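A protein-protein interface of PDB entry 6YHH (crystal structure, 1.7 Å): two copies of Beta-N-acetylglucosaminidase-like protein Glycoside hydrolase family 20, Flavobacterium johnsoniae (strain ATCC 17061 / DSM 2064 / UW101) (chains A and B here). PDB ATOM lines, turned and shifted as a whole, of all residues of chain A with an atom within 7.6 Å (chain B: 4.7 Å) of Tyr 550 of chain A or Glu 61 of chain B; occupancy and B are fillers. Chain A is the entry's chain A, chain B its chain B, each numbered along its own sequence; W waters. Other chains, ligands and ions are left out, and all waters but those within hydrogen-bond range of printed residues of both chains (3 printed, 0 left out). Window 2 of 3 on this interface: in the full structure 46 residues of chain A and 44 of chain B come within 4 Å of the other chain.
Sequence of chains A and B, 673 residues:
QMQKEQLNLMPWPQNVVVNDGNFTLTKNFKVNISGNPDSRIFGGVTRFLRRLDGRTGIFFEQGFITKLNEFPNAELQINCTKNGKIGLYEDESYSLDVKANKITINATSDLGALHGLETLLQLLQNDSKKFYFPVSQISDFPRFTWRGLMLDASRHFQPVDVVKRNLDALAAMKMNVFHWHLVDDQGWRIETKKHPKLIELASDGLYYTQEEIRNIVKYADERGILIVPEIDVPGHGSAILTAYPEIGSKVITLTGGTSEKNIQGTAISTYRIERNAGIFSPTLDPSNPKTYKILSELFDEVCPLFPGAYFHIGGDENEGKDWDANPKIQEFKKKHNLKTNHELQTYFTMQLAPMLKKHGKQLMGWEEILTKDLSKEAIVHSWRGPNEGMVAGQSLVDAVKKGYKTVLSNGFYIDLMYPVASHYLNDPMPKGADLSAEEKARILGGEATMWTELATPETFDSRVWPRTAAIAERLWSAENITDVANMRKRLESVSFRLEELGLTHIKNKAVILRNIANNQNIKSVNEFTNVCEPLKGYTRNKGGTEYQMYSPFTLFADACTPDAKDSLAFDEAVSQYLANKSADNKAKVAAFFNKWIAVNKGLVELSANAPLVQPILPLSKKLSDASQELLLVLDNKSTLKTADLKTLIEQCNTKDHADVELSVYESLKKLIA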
ATOM      1  N   ARG A 155     -21.843  21.371   5.163  1.00  0.00           N
ATOM      2  CA  ARG A 155     -20.505  21.233   5.710  1.00  0.00           C
ATOM      3  C   ARG A 155     -19.457  21.223   4.564  1.00  0.00           C
ATOM      4  O   ARG A 155     -18.557  22.024   4.523  1.00  0.00           O
ATOM      5  CB  ARG A 155     -20.410  19.985   6.576  1.00  0.00           C
ATOM      6  CG  ARG A 155     -20.961  20.181   7.994  1.00  0.00           C
ATOM      7  CD  ARG A 155     -22.325  20.809   8.076  1.00  0.00           C
ATOM      8  NE  ARG A 155     -22.788  20.919   9.483  1.00  0.00           N
ATOM      9  CZ  ARG A 155     -23.263  19.917  10.197  1.00  0.00           C
ATOM     10  NH1 ARG A 155     -23.457  18.701   9.664  1.00  0.00           N
ATOM     11  NH2 ARG A 155     -23.469  20.062  11.480  1.00  0.00           N
ATOM     12  N   HIS A 156     -19.627  20.331   3.621  1.00  0.00           N
ATOM     13  CA  HIS A 156     -19.007  20.372   2.310  1.00  0.00           C
ATOM     14  C   HIS A 156     -20.077  20.368   1.246  1.00  0.00           C
ATOM     15  O   HIS A 156     -20.879  19.474   1.160  1.00  0.00           O
ATOM     16  CB  HIS A 156     -18.081  19.178   1.993  1.00  0.00           C
ATOM     17  CG  HIS A 156     -16.733  19.264   2.647  1.00  0.00           C
ATOM     18  ND1 HIS A 156     -16.522  18.878   3.950  1.00  0.00           N
ATOM     19  CD2 HIS A 156     -15.548  19.748   2.203  1.00  0.00           C
ATOM     20  CE1 HIS A 156     -15.251  19.078   4.266  1.00  0.00           C
ATOM     21  NE2 HIS A 156     -14.639  19.594   3.232  1.00  0.00           N
ATOM     22  N   ASP A 204     -20.107  31.393   0.595  1.00  0.00           N
ATOM     23  CA  ASP A 204     -18.781  31.353  -0.078  1.00  0.00           C
ATOM     24  C   ASP A 204     -18.944  31.149  -1.585  1.00  0.00           C
ATOM     25  O   ASP A 204     -18.035  30.708  -2.286  1.00  0.00           O
ATOM     26  CB  ASP A 204     -17.876  30.228   0.482  1.00  0.00           C
ATOM     27  CG  ASP A 204     -17.537  30.392   1.928  1.00  0.00           C
ATOM     28  OD1 ASP A 204     -17.110  31.495   2.337  1.00  0.00           O
ATOM     29  OD2 ASP A 204     -17.679  29.367   2.672  1.00  0.00           O
ATOM     30  N   GLU A 274     -19.180  29.185   9.884  1.00  0.00           N
ATOM     31  CA  GLU A 274     -18.356  28.348  10.685  1.00  0.00           C
ATOM     32  C   GLU A 274     -17.447  27.434   9.810  1.00  0.00           C
ATOM     33  O   GLU A 274     -17.905  26.865   8.863  1.00  0.00           O
ATOM     34  CB  GLU A 274     -19.217  27.507  11.580  1.00  0.00           C
ATOM     35  CG  GLU A 274     -18.490  26.629  12.511  1.00  0.00           C
ATOM     36  CD  GLU A 274     -17.570  27.436  13.435  1.00  0.00           C
ATOM     37  OE1 GLU A 274     -17.882  28.534  13.958  1.00  0.00           O
ATOM     38  OE2 GLU A 274     -16.462  26.979  13.485  1.00  0.00           O
ATOM     39  N   ARG A 275     -16.159  27.346  10.193  1.00  0.00           N
ATOM     40  CA  ARG A 275     -15.165  26.589   9.413  1.00  0.00           C
ATOM     41  C   ARG A 275     -14.858  25.235  10.071  1.00  0.00           C
ATOM     42  O   ARG A 275     -14.204  24.374   9.411  1.00  0.00           O
ATOM     43  CB  ARG A 275     -13.867  27.380   9.229  1.00  0.00           C
ATOM     44  CG  ARG A 275     -14.071  28.746   8.575  1.00  0.00           C
ATOM     45  CD  ARG A 275     -14.820  28.614   7.280  1.00  0.00           C
ATOM     46  NE  ARG A 275     -14.927  29.893   6.601  1.00  0.00           N
ATOM     47  CZ  ARG A 275     -15.589  30.027   5.465  1.00  0.00           C
ATOM     48  NH1 ARG A 275     -16.176  29.015   4.948  1.00  0.00           N
ATOM     49  NH2 ARG A 275     -15.725  31.245   4.906  1.00  0.00           N
ATOM     50  N   ASN A 276     -15.196  25.090  11.327  1.00  0.00           N
ATOM     51  CA  ASN A 276     -14.922  23.854  12.098  1.00  0.00           C
ATOM     52  C   ASN A 276     -16.201  23.039  12.202  1.00  0.00           C
ATOM     53  O   ASN A 276     -17.281  23.474  11.835  1.00  0.00           O
ATOM     54  CB  ASN A 276     -14.499  24.222  13.529  1.00  0.00           C
ATOM     55  CG  ASN A 276     -13.114  24.816  13.567  1.00  0.00           C
ATOM     56  OD1 ASN A 276     -12.316  24.587  12.712  1.00  0.00           O
ATOM     57  ND2 ASN A 276     -12.835  25.543  14.571  1.00  0.00           N
ATOM     58  N   GLU A 453     -19.010  16.880   7.270  1.00  0.00           N
ATOM     59  CA  GLU A 453     -17.821  17.468   7.878  1.00  0.00           C
ATOM     60  C   GLU A 453     -16.543  16.936   7.278  1.00  0.00           C
ATOM     61  O   GLU A 453     -15.578  17.718   7.053  1.00  0.00           O
ATOM     62  CB  GLU A 453     -17.745  17.207   9.347  1.00  0.00           C
ATOM     63  CG  GLU A 453     -18.809  17.891  10.216  1.00  0.00           C
ATOM     64  CD  GLU A 453     -20.116  17.216  10.402  1.00  0.00           C
ATOM     65  OE1 GLU A 453     -20.491  16.340   9.569  1.00  0.00           O
ATOM     66  OE2 GLU A 453     -20.746  17.537  11.464  1.00  0.00           O
ATOM     67  N   THR A 456     -15.595  15.293   1.130  1.00  0.00           N
ATOM     68  CA  THR A 456     -15.615  16.241  -0.001  1.00  0.00           C
ATOM     69  C   THR A 456     -16.422  15.638  -1.107  1.00  0.00           C
ATOM     70  O   THR A 456     -16.779  14.470  -1.050  1.00  0.00           O
ATOM     71  CB  THR A 456     -14.186  16.435  -0.506  1.00  0.00           C
ATOM     72  OG1 THR A 456     -13.663  15.132  -0.860  1.00  0.00           O
ATOM     73  CG2 THR A 456     -13.299  17.075   0.589  1.00  0.00           C
ATOM     74  N   TYR A 547      -9.765  19.311  11.607  1.00  0.00           N
ATOM     75  CA  TYR A 547     -10.005  19.524  10.168  1.00  0.00           C
ATOM     76  C   TYR A 547     -11.028  20.654  10.054  1.00  0.00           C
ATOM     77  O   TYR A 547     -12.061  20.630  10.725  1.00  0.00           O
ATOM     78  CB  TYR A 547     -10.676  18.339   9.567  1.00  0.00           C
ATOM     79  CG  TYR A 547      -9.854  17.013   9.516  1.00  0.00           C
ATOM     80  CD1 TYR A 547      -9.687  16.216  10.640  1.00  0.00           C
ATOM     81  CD2 TYR A 547      -9.251  16.612   8.367  1.00  0.00           C
ATOM     82  CE1 TYR A 547      -8.973  15.038  10.602  1.00  0.00           C
ATOM     83  CE2 TYR A 547      -8.522  15.435   8.321  1.00  0.00           C
ATOM     84  CZ  TYR A 547      -8.400  14.641   9.402  1.00  0.00           C
ATOM     85  OH  TYR A 547      -7.736  13.387   9.317  1.00  0.00           O
ATOM     86  N   GLN A 548     -10.756  21.570   9.150  1.00  0.00           N
ATOM     87  CA  GLN A 548     -11.693  22.556   8.759  1.00  0.00           C
ATOM     88  C   GLN A 548     -12.429  22.130   7.505  1.00  0.00           C
ATOM     89  O   GLN A 548     -12.083  21.175   6.853  1.00  0.00           O
ATOM     90  CB  GLN A 548     -10.949  23.878   8.448  1.00  0.00           C
ATOM     91  CG  GLN A 548     -10.543  24.588   9.752  1.00  0.00           C
ATOM     92  CD  GLN A 548      -9.515  23.841  10.542  1.00  0.00           C
ATOM     93  OE1 GLN A 548      -8.421  23.515  10.032  1.00  0.00           O
ATOM     94  NE2 GLN A 548      -9.885  23.441  11.730  1.00  0.00           N
ATOM     95  N   MET A 549     -13.425  22.935   7.105  1.00  0.00           N
ATOM     96  CA  MET A 549     -14.238  22.608   5.949  1.00  0.00           C
ATOM     97  C   MET A 549     -13.451  22.861   4.602  1.00  0.00           C
ATOM     98  O   MET A 549     -14.014  22.663   3.556  1.00  0.00           O
ATOM     99  CB  MET A 549     -15.561  23.343   5.954  1.00  0.00           C
ATOM    100  CG  MET A 549     -16.529  23.042   7.126  1.00  0.00           C
ATOM    101  SD  MET A 549     -16.869  21.307   7.320  1.00  0.00           S
ATOM    102  CE  MET A 549     -15.818  20.901   8.707  1.00  0.00           C
ATOM    103  N   TYR A 550     -12.243  23.400   4.714  1.00  0.00           N
ATOM    104  CA  TYR A 550     -11.340  23.558   3.588  1.00  0.00           C
ATOM    105  C   TYR A 550     -10.015  22.748   3.726  1.00  0.00           C
ATOM    106  O   TYR A 550      -9.080  22.947   2.920  1.00  0.00           O
ATOM    107  CB  TYR A 550     -11.059  25.055   3.291  1.00  0.00           C
ATOM    108  CG  TYR A 550     -10.620  25.793   4.490  1.00  0.00           C
ATOM    109  CD1 TYR A 550      -9.328  25.703   5.013  1.00  0.00           C
ATOM    110  CD2 TYR A 550     -11.555  26.569   5.212  1.00  0.00           C
ATOM    111  CE1 TYR A 550      -8.935  26.398   6.168  1.00  0.00           C
ATOM    112  CE2 TYR A 550     -11.183  27.189   6.391  1.00  0.00           C
ATOM    113  CZ  TYR A 550      -9.898  27.138   6.843  1.00  0.00           C
ATOM    114  OH  TYR A 550      -9.594  27.834   7.992  1.00  0.00           O
ATOM    115  N   SER A 551      -9.960  21.807   4.656  1.00  0.00           N
ATOM    116  CA  SER A 551      -8.785  20.988   4.804  1.00  0.00           C
ATOM    117  C   SER A 551      -8.644  19.988   3.680  1.00  0.00           C
ATOM    118  O   SER A 551      -9.613  19.688   2.953  1.00  0.00           O
ATOM    119  CB  SER A 551      -8.889  20.228   6.126  1.00  0.00           C
ATOM    120  OG  SER A 551      -8.716  21.130   7.211  1.00  0.00           O
ATOM    121  N   PRO A 552      -7.430  19.423   3.492  1.00  0.00           N
ATOM    122  CA  PRO A 552      -7.229  18.461   2.448  1.00  0.00           C
ATOM    123  C   PRO A 552      -7.680  17.075   2.835  1.00  0.00           C
ATOM    124  O   PRO A 552      -7.188  16.530   3.797  1.00  0.00           O
ATOM    125  CB  PRO A 552      -5.744  18.520   2.185  1.00  0.00           C
ATOM    126  CG  PRO A 552      -5.170  18.857   3.495  1.00  0.00           C
ATOM    127  CD  PRO A 552      -6.152  19.765   4.146  1.00  0.00           C
ATOM    128  N   PHE A 553      -8.591  16.514   2.053  1.00  0.00           N
ATOM    129  CA  PHE A 553      -9.132  15.132   2.280  1.00  0.00           C
ATOM    130  C   PHE A 553      -8.629  14.252   1.166  1.00  0.00           C
ATOM    131  O   PHE A 553      -9.366  13.501   0.504  1.00  0.00           O
ATOM    132  CB  PHE A 553     -10.671  15.148   2.388  1.00  0.00           C
ATOM    133  CG  PHE A 553     -11.170  15.815   3.623  1.00  0.00           C
ATOM    134  CD1 PHE A 553     -11.342  15.115   4.767  1.00  0.00           C
ATOM    135  CD2 PHE A 553     -11.412  17.169   3.650  1.00  0.00           C
ATOM    136  CE1 PHE A 553     -11.708  15.744   5.957  1.00  0.00           C
ATOM    137  CE2 PHE A 553     -11.885  17.787   4.805  1.00  0.00           C
ATOM    138  CZ  PHE A 553     -12.029  17.084   5.959  1.00  0.00           C
ATOM    139  N   LYS B  30       1.786  31.217   3.478  1.00  0.00           N
ATOM    140  CA  LYS B  30       0.630  32.043   3.270  1.00  0.00           C
ATOM    141  C   LYS B  30       0.868  32.812   1.957  1.00  0.00           C
ATOM    142  O   LYS B  30       1.984  32.909   1.509  1.00  0.00           O
ATOM    143  CB  LYS B  30       0.450  33.011   4.441  1.00  0.00           C
ATOM    144  CG  LYS B  30       0.055  32.281   5.729  1.00  0.00           C
ATOM    145  CD  LYS B  30      -0.228  33.288   6.843  1.00  0.00           C
ATOM    146  CE  LYS B  30       1.055  33.906   7.315  1.00  0.00           C
ATOM    147  NZ  LYS B  30       2.062  32.967   7.952  1.00  0.00           N
ATOM    148  N   ARG B  50      -5.731  25.419  -2.240  1.00  0.00           N
ATOM    149  CA  ARG B  50      -6.409  24.115  -2.013  1.00  0.00           C
ATOM    150  C   ARG B  50      -5.680  22.980  -2.698  1.00  0.00           C
ATOM    151  O   ARG B  50      -5.467  21.887  -2.116  1.00  0.00           O
ATOM    152  CB  ARG B  50      -7.865  24.113  -2.465  1.00  0.00           C
ATOM    153  CG  ARG B  50      -8.734  25.101  -1.706  1.00  0.00           C
ATOM    154  CD  ARG B  50      -9.008  24.642  -0.262  1.00  0.00           C
ATOM    155  NE  ARG B  50      -7.998  24.981   0.717  1.00  0.00           N
ATOM    156  CZ  ARG B  50      -7.847  26.172   1.285  1.00  0.00           C
ATOM    157  NH1 ARG B  50      -8.605  27.192   0.859  1.00  0.00           N
ATOM    158  NH2 ARG B  50      -6.868  26.383   2.147  1.00  0.00           N
ATOM    159  N   PHE B  59      -2.029  21.454   5.755  1.00  0.00           N
ATOM    160  CA  PHE B  59      -3.166  22.080   6.444  1.00  0.00           C
ATOM    161  C   PHE B  59      -2.808  23.530   6.657  1.00  0.00           C
ATOM    162  O   PHE B  59      -2.563  24.055   7.824  1.00  0.00           O
ATOM    163  CB  PHE B  59      -3.565  21.406   7.767  1.00  0.00           C
ATOM    164  CG  PHE B  59      -4.255  20.062   7.602  1.00  0.00           C
ATOM    165  CD1 PHE B  59      -3.584  18.951   7.025  1.00  0.00           C
ATOM    166  CD2 PHE B  59      -5.569  19.889   8.079  1.00  0.00           C
ATOM    167  CE1 PHE B  59      -4.206  17.696   6.926  1.00  0.00           C
ATOM    168  CE2 PHE B  59      -6.159  18.605   7.995  1.00  0.00           C
ATOM    169  CZ  PHE B  59      -5.519  17.560   7.380  1.00  0.00           C
ATOM    170  N   PHE B  60      -2.818  24.220   5.516  1.00  0.00           N
ATOM    171  CA  PHE B  60      -2.532  25.650   5.514  1.00  0.00           C
ATOM    172  C   PHE B  60      -3.519  26.422   6.357  1.00  0.00           C
ATOM    173  O   PHE B  60      -4.712  26.104   6.452  1.00  0.00           O
ATOM    174  CB  PHE B  60      -2.442  26.241   4.094  1.00  0.00           C
ATOM    175  CG  PHE B  60      -1.326  25.610   3.223  1.00  0.00           C
ATOM    176  CD1 PHE B  60      -0.053  25.515   3.669  1.00  0.00           C
ATOM    177  CD2 PHE B  60      -1.632  25.095   2.031  1.00  0.00           C
ATOM    178  CE1 PHE B  60       0.972  24.976   2.909  1.00  0.00           C
ATOM    179  CE2 PHE B  60      -0.619  24.508   1.243  1.00  0.00           C
ATOM    180  CZ  PHE B  60       0.666  24.476   1.659  1.00  0.00           C
ATOM    181  N   GLU B  61      -3.012  27.571   6.871  1.00  0.00           N
ATOM    182  CA  GLU B  61      -3.808  28.454   7.725  1.00  0.00           C
ATOM    183  C   GLU B  61      -4.940  29.135   7.027  1.00  0.00           C
ATOM    184  O   GLU B  61      -6.094  29.239   7.576  1.00  0.00           O
ATOM    185  CB  GLU B  61      -2.867  29.499   8.363  1.00  0.00           C
ATOM    186  CG  GLU B  61      -3.615  30.550   9.156  1.00  0.00           C
ATOM    187  CD  GLU B  61      -2.714  31.647   9.761  1.00  0.00           C
ATOM    188  OE1 GLU B  61      -1.544  31.370  10.054  1.00  0.00           O
ATOM    189  OE2 GLU B  61      -3.231  32.757   9.963  1.00  0.00           O
ATOM    190  N   GLN B  62      -4.711  29.586   5.817  1.00  0.00           N
ATOM    191  CA  GLN B  62      -5.749  30.358   5.123  1.00  0.00           C
ATOM    192  C   GLN B  62      -6.871  29.452   4.567  1.00  0.00           C
ATOM    193  O   GLN B  62      -6.562  28.366   4.036  1.00  0.00           O
ATOM    194  CB  GLN B  62      -5.190  31.185   3.955  1.00  0.00           C
ATOM    195  CG  GLN B  62      -4.236  32.284   4.452  1.00  0.00           C
ATOM    196  CD  GLN B  62      -3.398  32.853   3.371  1.00  0.00           C
ATOM    197  OE1 GLN B  62      -2.508  32.230   2.917  1.00  0.00           O
ATOM    198  NE2 GLN B  62      -3.722  34.067   2.923  1.00  0.00           N
ATOM    199  N   GLY B  63      -8.104  29.980   4.582  1.00  0.00           N
ATOM    200  CA  GLY B  63      -9.258  29.333   3.966  1.00  0.00           C
ATOM    201  C   GLY B  63      -9.502  29.997   2.611  1.00  0.00           C
ATOM    202  O   GLY B  63      -8.696  29.857   1.715  1.00  0.00           O
ATOM    203  N   PHE B  71      -1.892  39.597   3.969  1.00  0.00           N
ATOM    204  CA  PHE B  71      -0.704  39.220   4.688  1.00  0.00           C
ATOM    205  C   PHE B  71       0.525  39.829   4.016  1.00  0.00           C
ATOM    206  O   PHE B  71       1.301  39.211   3.235  1.00  0.00           O
ATOM    207  CB  PHE B  71      -0.512  37.680   4.840  1.00  0.00           C
ATOM    208  CG  PHE B  71      -1.459  37.054   5.740  1.00  0.00           C
ATOM    209  CD1 PHE B  71      -1.330  37.179   7.128  1.00  0.00           C
ATOM    210  CD2 PHE B  71      -2.505  36.324   5.260  1.00  0.00           C
ATOM    211  CE1 PHE B  71      -2.230  36.565   7.997  1.00  0.00           C
ATOM    212  CE2 PHE B  71      -3.420  35.735   6.130  1.00  0.00           C
ATOM    213  CZ  PHE B  71      -3.284  35.841   7.483  1.00  0.00           C
HETATM  214  O   HOH W   1      -7.300  27.403   9.015  1.00  0.00           O
HETATM  215  O   HOH W   2      -6.403  24.854   8.810  1.00  0.00           O
HETATM  216  O   HOH W   3      -6.646  22.766   1.992  1.00  0.00           O
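The guanidinium group of Arg 50 of chain B lies within hydrogen-bond range of the backbone carbonyl oxygen of Tyr 550 of chain A (3.2 Å).
O of Gly 63 of chain B is in hydrogen-bond range of NH1 of Arg 50 of chain B, at 2.8 Å.
O of Gln 62 of chain B is in hydrogen-bond range of NH2 of Arg 50 of chain B, at 2.8 Å.
OG of Ser 551 of chain A sits at hydrogen-bond distance from N of Gln 548 of chain A (2.8 Å).
Among the printed residues, merely in contact across the chains: Ser 551 of chain A with Phe 59 of chain B, Tyr 550 of chain A with Gly 63 of chain B, Tyr 547 of chain A with Phe 59 of chain B, Pro 552 of chain A with Phe 59 of chain B, Tyr 550 of chain A with Gln 62 of chain B and Tyr 550 of chain A with Glu 61 of chain B.
Of chain B, only Arg 50, Glu 61, Gln 62 and Gly 63 come within 4 Å of Tyr 550 of chain A.
Glu 61 of chain B touches just one residue of chain A: Tyr 550.
Printed residues of chain B within 4 Å of Pro 552 of chain A: Phe 59 (3.7 Å).
Of the printed residues of chain A, Gly 63 of chain B touches Tyr 550.
Of the printed residues of chain B, Ser 551 of chain A touches Phe 59.
Printed residues of chain A within 4 Å of Gln 62 of chain B: Tyr 550.
Lys 30 of chain B touches none of the printed residues of chain A.
Phe 553 of chain A touches none of the printed residues of chain B.
The nearest printed residue of chain A that does not touch Arg 50 of chain B is Ser 551 of chain A (5.4 Å).
Printed residues of chain B that touch a printed residue of chain A: Arg 50, Phe 59, Glu 61, Gln 62 and Gly 63.
Hydrophobic or aromatic side chains of chain B within 4 Å of the printed part of chain A: Phe 59.
Printed residues of chain A that touch a printed residue of chain B: Tyr 547, Tyr 550, Ser 551 and Pro 552.
Hydrophobic or aromatic side chains of chain A that line the printed part of chain B: Tyr 547, Tyr 550 and Pro 552.
Among the printed residues, 7 pairs touch across the chains.
No position is printed for both chains.
Water W1 bridges OH of Tyr 550 of chain A (2.5 Å) and O of Glu 61 of chain B (2.6 Å).
Water W3 bridges O of Tyr 550 of chain A (2.6 Å) and NE of Arg 50 of chain B (2.9 Å).
Water W2 lies within hydrogen-bond range of the side-chain amide oxygen (OE1) of Gln 548 of chain A (2.7 Å) and the backbone carbonyl oxygen (O) of Phe 60 of chain B (3.2 Å).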
